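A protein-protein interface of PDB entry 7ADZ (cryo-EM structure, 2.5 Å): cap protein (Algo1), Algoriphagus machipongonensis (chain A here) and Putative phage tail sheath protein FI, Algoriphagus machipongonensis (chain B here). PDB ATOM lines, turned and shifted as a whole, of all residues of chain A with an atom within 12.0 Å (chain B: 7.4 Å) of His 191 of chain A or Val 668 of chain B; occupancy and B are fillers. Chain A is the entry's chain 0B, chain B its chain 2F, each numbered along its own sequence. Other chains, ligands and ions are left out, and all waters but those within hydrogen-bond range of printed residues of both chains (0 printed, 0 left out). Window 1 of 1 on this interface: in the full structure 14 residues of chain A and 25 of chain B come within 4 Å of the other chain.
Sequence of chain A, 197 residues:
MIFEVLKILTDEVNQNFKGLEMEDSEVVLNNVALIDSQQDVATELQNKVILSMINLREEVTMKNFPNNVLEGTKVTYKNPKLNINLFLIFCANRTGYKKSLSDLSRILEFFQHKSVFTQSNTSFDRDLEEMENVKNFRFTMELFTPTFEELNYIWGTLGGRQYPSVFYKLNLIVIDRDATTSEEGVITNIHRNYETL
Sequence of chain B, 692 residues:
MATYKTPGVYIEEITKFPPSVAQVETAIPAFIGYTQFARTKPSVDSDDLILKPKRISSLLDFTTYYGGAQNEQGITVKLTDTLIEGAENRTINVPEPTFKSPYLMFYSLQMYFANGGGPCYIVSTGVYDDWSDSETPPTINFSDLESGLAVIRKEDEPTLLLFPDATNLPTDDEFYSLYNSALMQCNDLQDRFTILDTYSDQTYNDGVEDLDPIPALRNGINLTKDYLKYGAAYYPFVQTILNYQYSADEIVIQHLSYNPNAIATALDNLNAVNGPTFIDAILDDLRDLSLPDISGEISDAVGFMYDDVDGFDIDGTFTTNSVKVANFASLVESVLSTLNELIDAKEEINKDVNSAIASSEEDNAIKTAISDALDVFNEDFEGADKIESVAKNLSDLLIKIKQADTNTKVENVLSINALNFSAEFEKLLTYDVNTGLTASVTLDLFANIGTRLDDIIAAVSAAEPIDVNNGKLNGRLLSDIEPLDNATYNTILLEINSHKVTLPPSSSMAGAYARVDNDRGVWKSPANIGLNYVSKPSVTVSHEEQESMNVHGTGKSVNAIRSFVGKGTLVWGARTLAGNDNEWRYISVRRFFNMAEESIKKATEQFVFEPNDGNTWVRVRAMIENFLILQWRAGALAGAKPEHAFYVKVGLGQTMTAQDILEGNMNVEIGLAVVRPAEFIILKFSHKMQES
Of the printed residues of chain B, Thr 188 of chain A touches Glu 663 and Gly 664. Printed residues of chain B within 4 Å of Ile 190 of chain A: Met 666. His 191 of chain A touches four residues of chain B. Of the printed residues of chain B, Asn 193 of chain A touches Val 668, Glu 669 and Ile 670. Thr 196 of chain A touches none of the printed residues of chain B. Of the printed residues of chain A, Ile 600 of chain B touches Tyr 194 (3.9 Å). No residue of chain A comes within 4 Å of Thr 655 of chain B. Printed residues of chain A within 4 Å of Glu 663 of chain B: Thr 188 (3.9 Å). Asn 665 of chain B touches just these residues of chain A: Asn 189 (3.1 Å) and His 191 (3.9 Å). Of the printed residues of chain A, Met 666 of chain B touches Asn 189, Ile 190 and His 191. Asn 667 of chain B touches just one residue of chain A: His 191. Val 668 of chain B touches just these residues of chain A: His 191 (3.0 Å), Arg 192 (3.6 Å) and Asn 193 (3.1 Å). Glu 669 of chain B touches just these residues of chain A: Asn 193 and Glu 195. The nearest residue of chain A that does not touch Val 668 of chain B is Ile 190 of chain A (5.4 Å).
Printed residues of chain B that touch a printed residue of chain A: Ile 600, Thr 604, Glu 663, Gly 664, Asn 665, Met 666, Asn 667, Val 668, Glu 669 and Ile 670. Hydrophobic or aromatic side chains of chain B within 4 Å of the printed part of chain A: Ile 600. Of the 11 printed residues of chain A, 10 touch a printed residue of chain B. Printed residues of chain A that touch a printed residue of chain B: Val 186, Ile 187, Thr 188, Asn 189, Ile 190, His 191, Arg 192, Asn 193, Tyr 194 and Glu 195. Hydrophobic or aromatic side chains of chain A that line the printed part of chain B: His 191 and Tyr 194. Among the printed residues, 21 pairs touch across the chains. Among the printed residues, no Asp or Glu carboxylate lies within 4 Å of a Lys or Arg side-chain nitrogen of the other chain.
N of Thr 188 of chain A is in hydrogen-bond range of O of Gly 664 of chain B (3.0 Å). The backbone NH (N) of Asn 189 of chain A is in hydrogen-bond range of the backbone carbonyl oxygen (O) of Gly 664 of chain B (3.2 Å). ND2 of Asn 189 of chain A sits close to OD1 of Asn 665 of chain B. The backbone carbonyl oxygen (O) of Asn 189 of chain A sits at hydrogen-bond distance from the backbone NH (N) of Met 666 of chain B, at 2.9 Å. The backbone carbonyl oxygen of Met 666 of chain B sits at hydrogen-bond distance from the backbone NH of His 191 of chain A (3.2 Å). O of His 191 of chain A sits at hydrogen-bond distance from N of Val 668 of chain B (3.0 Å). The side-chain hydroxyl (OG1) of Thr 604 of chain B is in hydrogen-bond range of the guanidinium group (NH1) of Arg 192 of chain A (3.0 Å). O of Val 668 of chain B sits at hydrogen-bond distance from N of Asn 193 of chain A. N of Ile 670 of chain B is in hydrogen-bond range of O of Asn 193 of chain A (3.0 Å). The backbone NH (N) of Glu 195 of chain A sits at hydrogen-bond distance from the backbone carbonyl oxygen (O) of Ile 670 of chain B, at 3.1 Å.
The side-chain amide nitrogen of Asn 189 of chain A sits at hydrogen-bond distance from the side-chain hydroxyl of Thr 188 of chain A (3.2 Å). The side-chain amino group (NZ) of Lys 649 of chain B lies within salt-bridge range of the side-chain carboxylate (OE1) of Glu 669 of chain B. OG1 of Thr 655 of chain B is in hydrogen-bond range of O of Asn 667 of chain B. O of Asp 660 of chain B sits at hydrogen-bond distance from N of Asn 665 of chain B, at 3.0 Å. OE1 of Glu 663 of chain B is in hydrogen-bond range of ND2 of Asn 665 of chain B.
Among the printed residues, pairs that only touch across the chains: Val 186 of chain A with Gly 664 of chain B, Ile 187 of chain A with Gly 664 of chain B, Thr 188 of chain A with Glu 663 of chain B, Ile 190 of chain A with Met 666 of chain B, His 191 of chain A with Asn 665 of chain B, His 191 of chain A with Asn 667 of chain B, Arg 192 of chain A with Val 668 of chain B, Asn 193 of chain A with Glu 669 of chain B, Tyr 194 of chain A with Ile 600 of chain B, Tyr 194 of chain A with Ile 670 of chain B and Glu 195 of chain A with Glu 669 of chain B.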
ATOM      1  N   VAL A 186      15.356  40.066  18.665  1.00  0.00           N
ATOM      2  CA  VAL A 186      14.538  39.331  17.699  1.00  0.00           C
ATOM      3  C   VAL A 186      15.354  38.955  16.463  1.00  0.00           C
ATOM      4  O   VAL A 186      16.509  39.353  16.283  1.00  0.00           O
ATOM      5  CB  VAL A 186      13.288  40.140  17.313  1.00  0.00           C
ATOM      6  CG1 VAL A 186      12.551  40.585  18.549  1.00  0.00           C
ATOM      7  CG2 VAL A 186      13.668  41.333  16.456  1.00  0.00           C
ATOM      8  N   ILE A 187      14.722  38.166  15.595  1.00  0.00           N
ATOM      9  CA  ILE A 187      15.340  37.672  14.369  1.00  0.00           C
ATOM     10  C   ILE A 187      15.448  38.807  13.359  1.00  0.00           C
ATOM     11  O   ILE A 187      14.452  39.462  13.033  1.00  0.00           O
ATOM     12  CB  ILE A 187      14.530  36.497  13.800  1.00  0.00           C
ATOM     13  CG1 ILE A 187      14.585  35.307  14.755  1.00  0.00           C
ATOM     14  CG2 ILE A 187      15.021  36.102  12.419  1.00  0.00           C
ATOM     15  CD1 ILE A 187      13.709  34.148  14.352  1.00  0.00           C
ATOM     16  N   THR A 188      16.666  39.051  12.857  1.00  0.00           N
ATOM     17  CA  THR A 188      16.885  40.055  11.820  1.00  0.00           C
ATOM     18  C   THR A 188      17.682  39.572  10.612  1.00  0.00           C
ATOM     19  O   THR A 188      17.760  40.314   9.629  1.00  0.00           O
ATOM     20  CB  THR A 188      17.585  41.300  12.397  1.00  0.00           C
ATOM     21  OG1 THR A 188      18.795  40.921  13.063  1.00  0.00           O
ATOM     22  CG2 THR A 188      16.688  42.063  13.365  1.00  0.00           C
ATOM     23  N   ASN A 189      18.275  38.378  10.639  1.00  0.00           N
ATOM     24  CA  ASN A 189      19.028  37.844   9.507  1.00  0.00           C
ATOM     25  C   ASN A 189      18.662  36.384   9.289  1.00  0.00           C
ATOM     26  O   ASN A 189      18.647  35.600  10.241  1.00  0.00           O
ATOM     27  CB  ASN A 189      20.541  37.961   9.727  1.00  0.00           C
ATOM     28  CG  ASN A 189      20.982  39.369  10.058  1.00  0.00           C
ATOM     29  OD1 ASN A 189      21.151  40.199   9.174  1.00  0.00           O
ATOM     30  ND2 ASN A 189      21.190  39.637  11.338  1.00  0.00           N
ATOM     31  N   ILE A 190      18.376  36.016   8.041  1.00  0.00           N
ATOM     32  CA  ILE A 190      17.989  34.657   7.674  1.00  0.00           C
ATOM     33  C   ILE A 190      18.930  34.154   6.585  1.00  0.00           C
ATOM     34  O   ILE A 190      19.154  34.843   5.585  1.00  0.00           O
ATOM     35  CB  ILE A 190      16.519  34.592   7.209  1.00  0.00           C
ATOM     36  CG1 ILE A 190      15.588  35.151   8.287  1.00  0.00           C
ATOM     37  CG2 ILE A 190      16.117  33.165   6.879  1.00  0.00           C
ATOM     38  CD1 ILE A 190      14.182  35.399   7.841  1.00  0.00           C
ATOM     39  N   HIS A 191      19.481  32.958   6.783  1.00  0.00           N
ATOM     40  CA  HIS A 191      20.400  32.326   5.842  1.00  0.00           C
ATOM     41  C   HIS A 191      19.887  30.934   5.502  1.00  0.00           C
ATOM     42  O   HIS A 191      19.484  30.186   6.395  1.00  0.00           O
ATOM     43  CB  HIS A 191      21.814  32.226   6.423  1.00  0.00           C
ATOM     44  CG  HIS A 191      22.345  33.514   6.965  1.00  0.00           C
ATOM     45  ND1 HIS A 191      23.274  34.275   6.293  1.00  0.00           N
ATOM     46  CD2 HIS A 191      22.091  34.167   8.123  1.00  0.00           C
ATOM     47  CE1 HIS A 191      23.563  35.345   7.010  1.00  0.00           C
ATOM     48  NE2 HIS A 191      22.858  35.304   8.125  1.00  0.00           N
ATOM     49  N   ARG A 192      19.901  30.586   4.216  1.00  0.00           N
ATOM     50  CA  ARG A 192      19.411  29.299   3.739  1.00  0.00           C
ATOM     51  C   ARG A 192      20.474  28.619   2.889  1.00  0.00           C
ATOM     52  O   ARG A 192      21.030  29.233   1.975  1.00  0.00           O
ATOM     53  CB  ARG A 192      18.110  29.463   2.944  1.00  0.00           C
ATOM     54  CG  ARG A 192      16.922  29.916   3.784  1.00  0.00           C
ATOM     55  CD  ARG A 192      15.608  29.907   3.019  1.00  0.00           C
ATOM     56  NE  ARG A 192      15.537  30.926   1.976  1.00  0.00           N
ATOM     57  CZ  ARG A 192      15.132  32.176   2.170  1.00  0.00           C
ATOM     58  NH1 ARG A 192      14.766  32.581   3.373  1.00  0.00           N
ATOM     59  NH2 ARG A 192      15.102  33.028   1.159  1.00  0.00           N
ATOM     60  N   ASN A 193      20.747  27.351   3.186  1.00  0.00           N
ATOM     61  CA  ASN A 193      21.743  26.555   2.478  1.00  0.00           C
ATOM     62  C   ASN A 193      21.085  25.320   1.883  1.00  0.00           C
ATOM     63  O   ASN A 193      20.337  24.621   2.568  1.00  0.00           O
ATOM     64  CB  ASN A 193      22.880  26.142   3.412  1.00  0.00           C
ATOM     65  CG  ASN A 193      23.718  27.313   3.848  1.00  0.00           C
ATOM     66  OD1 ASN A 193      23.673  27.729   5.005  1.00  0.00           O
ATOM     67  ND2 ASN A 193      24.511  27.844   2.930  1.00  0.00           N
ATOM     68  N   TYR A 194      21.372  25.056   0.613  1.00  0.00           N
ATOM     69  CA  TYR A 194      20.766  23.962  -0.131  1.00  0.00           C
ATOM     70  C   TYR A 194      21.854  23.024  -0.631  1.00  0.00           C
ATOM     71  O   TYR A 194      22.933  23.471  -1.029  1.00  0.00           O
ATOM     72  CB  TYR A 194      19.948  24.480  -1.320  1.00  0.00           C
ATOM     73  CG  TYR A 194      18.723  25.287  -0.948  1.00  0.00           C
ATOM     74  CD1 TYR A 194      17.472  24.691  -0.876  1.00  0.00           C
ATOM     75  CD2 TYR A 194      18.813  26.649  -0.691  1.00  0.00           C
ATOM     76  CE1 TYR A 194      16.352  25.423  -0.545  1.00  0.00           C
ATOM     77  CE2 TYR A 194      17.701  27.388  -0.354  1.00  0.00           C
ATOM     78  CZ  TYR A 194      16.476  26.774  -0.284  1.00  0.00           C
ATOM     79  OH  TYR A 194      15.366  27.507   0.046  1.00  0.00           O
ATOM     80  N   GLU A 195      21.577  21.727  -0.603  1.00  0.00           N
ATOM     81  CA  GLU A 195      22.491  20.746  -1.170  1.00  0.00           C
ATOM     82  C   GLU A 195      21.692  19.683  -1.904  1.00  0.00           C
ATOM     83  O   GLU A 195      20.508  19.473  -1.636  1.00  0.00           O
ATOM     84  CB  GLU A 195      23.387  20.106  -0.098  1.00  0.00           C
ATOM     85  CG  GLU A 195      22.767  18.964   0.673  1.00  0.00           C
ATOM     86  CD  GLU A 195      23.773  18.240   1.543  1.00  0.00           C
ATOM     87  OE1 GLU A 195      24.166  18.797   2.588  1.00  0.00           O
ATOM     88  OE2 GLU A 195      24.174  17.113   1.181  1.00  0.00           O
ATOM     89  N   THR A 196      22.349  19.028  -2.857  1.00  0.00           N
ATOM     90  CA  THR A 196      21.732  17.980  -3.660  1.00  0.00           C
ATOM     91  C   THR A 196      22.045  16.639  -3.005  1.00  0.00           C
ATOM     92  O   THR A 196      23.204  16.218  -2.956  1.00  0.00           O
ATOM     93  CB  THR A 196      22.224  18.021  -5.106  1.00  0.00           C
ATOM     94  OG1 THR A 196      21.768  19.227  -5.727  1.00  0.00           O
ATOM     95  CG2 THR A 196      21.679  16.841  -5.882  1.00  0.00           C
ATOM     96  N   ILE B 600       9.699  27.898   0.154  1.00  0.00           N
ATOM     97  CA  ILE B 600      10.395  27.868   1.425  1.00  0.00           C
ATOM     98  C   ILE B 600      10.637  29.284   1.916  1.00  0.00           C
ATOM     99  O   ILE B 600      10.419  29.574   3.089  1.00  0.00           O
ATOM    100  CB  ILE B 600      11.656  27.010   1.335  1.00  0.00           C
ATOM    101  CG1 ILE B 600      11.178  25.532   1.134  1.00  0.00           C
ATOM    102  CG2 ILE B 600      12.507  27.174   2.612  1.00  0.00           C
ATOM    103  CD1 ILE B 600      12.225  24.553   0.721  1.00  0.00           C
ATOM    104  N   THR B 604       9.675  31.112   5.692  1.00  0.00           N
ATOM    105  CA  THR B 604      10.546  31.629   6.746  1.00  0.00           C
ATOM    106  C   THR B 604      10.384  33.134   6.966  1.00  0.00           C
ATOM    107  O   THR B 604      10.592  33.619   8.080  1.00  0.00           O
ATOM    108  CB  THR B 604      12.038  31.291   6.483  1.00  0.00           C
ATOM    109  OG1 THR B 604      12.488  31.915   5.281  1.00  0.00           O
ATOM    110  CG2 THR B 604      12.211  29.775   6.340  1.00  0.00           C
ATOM    111  N   VAL B 620       9.164  26.498  12.233  1.00  0.00           N
ATOM    112  CA  VAL B 620       9.807  26.657  10.939  1.00  0.00           C
ATOM    113  C   VAL B 620      10.067  25.306  10.310  1.00  0.00           C
ATOM    114  O   VAL B 620       9.768  25.093   9.130  1.00  0.00           O
ATOM    115  CB  VAL B 620      11.138  27.437  11.092  1.00  0.00           C
ATOM    116  CG1 VAL B 620      11.955  27.423   9.803  1.00  0.00           C
ATOM    117  CG2 VAL B 620      10.831  28.858  11.437  1.00  0.00           C
ATOM    118  N   ARG B 621      10.625  24.391  11.088  1.00  0.00           N
ATOM    119  CA  ARG B 621      10.900  23.081  10.569  1.00  0.00           C
ATOM    120  C   ARG B 621       9.639  22.366  10.112  1.00  0.00           C
ATOM    121  O   ARG B 621       9.626  21.787   9.024  1.00  0.00           O
ATOM    122  CB  ARG B 621      11.627  22.247  11.586  1.00  0.00           C
ATOM    123  CG  ARG B 621      11.948  20.867  11.116  1.00  0.00           C
ATOM    124  CD  ARG B 621      12.770  20.153  12.054  1.00  0.00           C
ATOM    125  NE  ARG B 621      12.855  18.780  11.682  1.00  0.00           N
ATOM    126  CZ  ARG B 621      13.535  17.830  12.315  1.00  0.00           C
ATOM    127  NH1 ARG B 621      14.254  18.093  13.386  1.00  0.00           N
ATOM    128  NH2 ARG B 621      13.452  16.617  11.823  1.00  0.00           N
ATOM    129  N   ILE B 624       8.329  23.614   6.641  1.00  0.00           N
ATOM    130  CA  ILE B 624       9.146  23.195   5.522  1.00  0.00           C
ATOM    131  C   ILE B 624       8.955  21.719   5.223  1.00  0.00           C
ATOM    132  O   ILE B 624       8.830  21.345   4.052  1.00  0.00           O
ATOM    133  CB  ILE B 624      10.622  23.512   5.751  1.00  0.00           C
ATOM    134  CG1 ILE B 624      10.796  25.035   5.797  1.00  0.00           C
ATOM    135  CG2 ILE B 624      11.463  22.909   4.585  1.00  0.00           C
ATOM    136  CD1 ILE B 624      12.121  25.503   6.310  1.00  0.00           C
ATOM    137  N   VAL B 648      15.733  18.440   6.770  1.00  0.00           N
ATOM    138  CA  VAL B 648      15.707  19.835   7.204  1.00  0.00           C
ATOM    139  C   VAL B 648      16.327  19.965   8.601  1.00  0.00           C
ATOM    140  O   VAL B 648      15.962  19.204   9.490  1.00  0.00           O
ATOM    141  CB  VAL B 648      14.244  20.359   7.248  1.00  0.00           C
ATOM    142  CG1 VAL B 648      14.196  21.843   7.685  1.00  0.00           C
ATOM    143  CG2 VAL B 648      13.579  20.182   5.893  1.00  0.00           C
ATOM    144  N   LYS B 649      17.235  20.917   8.802  1.00  0.00           N
ATOM    145  CA  LYS B 649      17.827  21.156  10.126  1.00  0.00           C
ATOM    146  C   LYS B 649      17.777  22.623  10.541  1.00  0.00           C
ATOM    147  O   LYS B 649      18.209  23.506   9.797  1.00  0.00           O
ATOM    148  CB  LYS B 649      19.291  20.750  10.139  1.00  0.00           C
ATOM    149  CG  LYS B 649      19.602  19.296   9.983  1.00  0.00           C
ATOM    150  CD  LYS B 649      21.043  19.136   9.507  1.00  0.00           C
ATOM    151  CE  LYS B 649      22.087  19.544  10.544  1.00  0.00           C
ATOM    152  NZ  LYS B 649      23.471  19.455   9.967  1.00  0.00           N
ATOM    153  N   VAL B 650      17.200  22.903  11.714  1.00  0.00           N
ATOM    154  CA  VAL B 650      17.155  24.275  12.228  1.00  0.00           C
ATOM    155  C   VAL B 650      17.405  24.275  13.735  1.00  0.00           C
ATOM    156  O   VAL B 650      16.689  23.576  14.446  1.00  0.00           O
ATOM    157  CB  VAL B 650      15.750  24.912  12.010  1.00  0.00           C
ATOM    158  CG1 VAL B 650      15.740  26.401  12.482  1.00  0.00           C
ATOM    159  CG2 VAL B 650      15.335  24.786  10.585  1.00  0.00           C
ATOM    160  N   GLY B 651      18.306  25.099  14.259  1.00  0.00           N
ATOM    161  CA  GLY B 651      18.379  25.174  15.719  1.00  0.00           C
ATOM    162  C   GLY B 651      19.751  25.237  16.361  1.00  0.00           C
ATOM    163  O   GLY B 651      20.779  24.848  15.780  1.00  0.00           O
ATOM    164  N   THR B 655      22.460  24.045  13.584  1.00  0.00           N
ATOM    165  CA  THR B 655      22.829  25.023  12.575  1.00  0.00           C
ATOM    166  C   THR B 655      23.300  26.345  13.185  1.00  0.00           C
ATOM    167  O   THR B 655      23.899  27.166  12.487  1.00  0.00           O
ATOM    168  CB  THR B 655      21.671  25.304  11.605  1.00  0.00           C
ATOM    169  OG1 THR B 655      20.536  25.877  12.315  1.00  0.00           O
ATOM    170  CG2 THR B 655      21.238  24.031  10.919  1.00  0.00           C
ATOM    171  N   MET B 656      23.038  26.551  14.478  1.00  0.00           N
ATOM    172  CA  MET B 656      23.382  27.795  15.160  1.00  0.00           C
ATOM    173  C   MET B 656      24.232  27.644  16.405  1.00  0.00           C
ATOM    174  O   MET B 656      24.204  26.623  17.107  1.00  0.00           O
ATOM    175  CB  MET B 656      22.122  28.554  15.540  1.00  0.00           C
ATOM    176  CG  MET B 656      21.365  29.066  14.388  1.00  0.00           C
ATOM    177  SD  MET B 656      19.866  29.871  14.831  1.00  0.00           S
ATOM    178  CE  MET B 656      18.767  28.574  15.041  1.00  0.00           C
ATOM    179  N   ASP B 660      25.161  33.357  17.059  1.00  0.00           N
ATOM    180  CA  ASP B 660      24.060  33.637  16.161  1.00  0.00           C
ATOM    181  C   ASP B 660      22.904  34.123  16.982  1.00  0.00           C
ATOM    182  O   ASP B 660      22.119  34.973  16.548  1.00  0.00           O
ATOM    183  CB  ASP B 660      23.640  32.373  15.422  1.00  0.00           C
ATOM    184  CG  ASP B 660      24.663  31.881  14.460  1.00  0.00           C
ATOM    185  OD1 ASP B 660      25.012  32.606  13.539  1.00  0.00           O
ATOM    186  OD2 ASP B 660      25.100  30.748  14.629  1.00  0.00           O
ATOM    187  N   GLU B 663      23.800  37.795  17.555  1.00  0.00           N
ATOM    188  CA  GLU B 663      23.624  38.617  16.360  1.00  0.00           C
ATOM    189  C   GLU B 663      22.175  38.729  15.891  1.00  0.00           C
ATOM    190  O   GLU B 663      21.775  39.758  15.349  1.00  0.00           O
ATOM    191  CB  GLU B 663      24.493  38.100  15.220  1.00  0.00           C
ATOM    192  CG  GLU B 663      25.977  38.298  15.450  1.00  0.00           C
ATOM    193  CD  GLU B 663      26.863  37.800  14.326  1.00  0.00           C
ATOM    194  OE1 GLU B 663      26.370  37.441  13.266  1.00  0.00           O
ATOM    195  OE2 GLU B 663      28.052  37.733  14.557  1.00  0.00           O
ATOM    196  N   GLY B 664      21.387  37.672  16.080  1.00  0.00           N
ATOM    197  CA  GLY B 664      20.002  37.655  15.637  1.00  0.00           C
ATOM    198  C   GLY B 664      19.821  36.884  14.337  1.00  0.00           C
ATOM    199  O   GLY B 664      18.953  37.210  13.531  1.00  0.00           O
ATOM    200  N   ASN B 665      20.660  35.880  14.115  1.00  0.00           N
ATOM    201  CA  ASN B 665      20.586  35.085  12.900  1.00  0.00           C
ATOM    202  C   ASN B 665      19.755  33.816  13.071  1.00  0.00           C
ATOM    203  O   ASN B 665      19.697  33.243  14.161  1.00  0.00           O
ATOM    204  CB  ASN B 665      21.973  34.658  12.487  1.00  0.00           C
ATOM    205  CG  ASN B 665      22.900  35.772  12.249  1.00  0.00           C
ATOM    206  OD1 ASN B 665      22.552  36.845  11.749  1.00  0.00           O
ATOM    207  ND2 ASN B 665      24.128  35.525  12.622  1.00  0.00           N
ATOM    208  N   MET B 666      19.180  33.324  11.971  1.00  0.00           N
ATOM    209  CA  MET B 666      18.539  32.015  11.975  1.00  0.00           C
ATOM    210  C   MET B 666      19.050  31.257  10.764  1.00  0.00           C
ATOM    211  O   MET B 666      18.918  31.723   9.636  1.00  0.00           O
ATOM    212  CB  MET B 666      17.014  32.090  11.968  1.00  0.00           C
ATOM    213  CG  MET B 666      16.337  30.683  12.023  1.00  0.00           C
ATOM    214  SD  MET B 666      14.532  30.696  12.107  1.00  0.00           S
ATOM    215  CE  MET B 666      14.048  31.064  10.425  1.00  0.00           C
ATOM    216  N   ASN B 667      19.628  30.089  11.003  1.00  0.00           N
ATOM    217  CA  ASN B 667      20.236  29.284   9.952  1.00  0.00           C
ATOM    218  C   ASN B 667      19.436  28.029   9.595  1.00  0.00           C
ATOM    219  O   ASN B 667      19.167  27.188  10.450  1.00  0.00           O
ATOM    220  CB  ASN B 667      21.646  28.913  10.356  1.00  0.00           C
ATOM    221  CG  ASN B 667      22.547  30.107  10.557  1.00  0.00           C
ATOM    222  OD1 ASN B 667      22.394  31.159   9.927  1.00  0.00           O
ATOM    223  ND2 ASN B 667      23.512  29.948  11.422  1.00  0.00           N
ATOM    224  N   VAL B 668      19.048  27.890   8.334  1.00  0.00           N
ATOM    225  CA  VAL B 668      18.267  26.721   7.927  1.00  0.00           C
ATOM    226  C   VAL B 668      19.008  25.893   6.865  1.00  0.00           C
ATOM    227  O   VAL B 668      19.376  26.413   5.815  1.00  0.00           O
ATOM    228  CB  VAL B 668      16.895  27.179   7.365  1.00  0.00           C
ATOM    229  CG1 VAL B 668      16.066  25.973   6.921  1.00  0.00           C
ATOM    230  CG2 VAL B 668      16.140  28.018   8.421  1.00  0.00           C
ATOM    231  N   GLU B 669      19.215  24.602   7.140  1.00  0.00           N
ATOM    232  CA  GLU B 669      19.900  23.698   6.200  1.00  0.00           C
ATOM    233  C   GLU B 669      18.943  22.676   5.575  1.00  0.00           C
ATOM    234  O   GLU B 669      18.211  21.990   6.287  1.00  0.00           O
ATOM    235  CB  GLU B 669      21.044  22.961   6.889  1.00  0.00           C
ATOM    236  CG  GLU B 669      21.798  22.005   5.978  1.00  0.00           C
ATOM    237  CD  GLU B 669      22.880  21.192   6.661  1.00  0.00           C
ATOM    238  OE1 GLU B 669      23.226  21.468   7.793  1.00  0.00           O
ATOM    239  OE2 GLU B 669      23.329  20.244   6.058  1.00  0.00           O
ATOM    240  N   ILE B 670      18.919  22.591   4.234  1.00  0.00           N
ATOM    241  CA  ILE B 670      18.019  21.664   3.518  1.00  0.00           C
ATOM    242  C   ILE B 670      18.713  20.834   2.429  1.00  0.00           C
ATOM    243  O   ILE B 670      19.507  21.369   1.658  1.00  0.00           O
ATOM    244  CB  ILE B 670      16.833  22.432   2.874  1.00  0.00           C
ATOM    245  CG1 ILE B 670      16.093  23.186   3.977  1.00  0.00           C
ATOM    246  CG2 ILE B 670      15.858  21.448   2.125  1.00  0.00           C
ATOM    247  CD1 ILE B 670      15.057  24.110   3.524  1.00  0.00           C
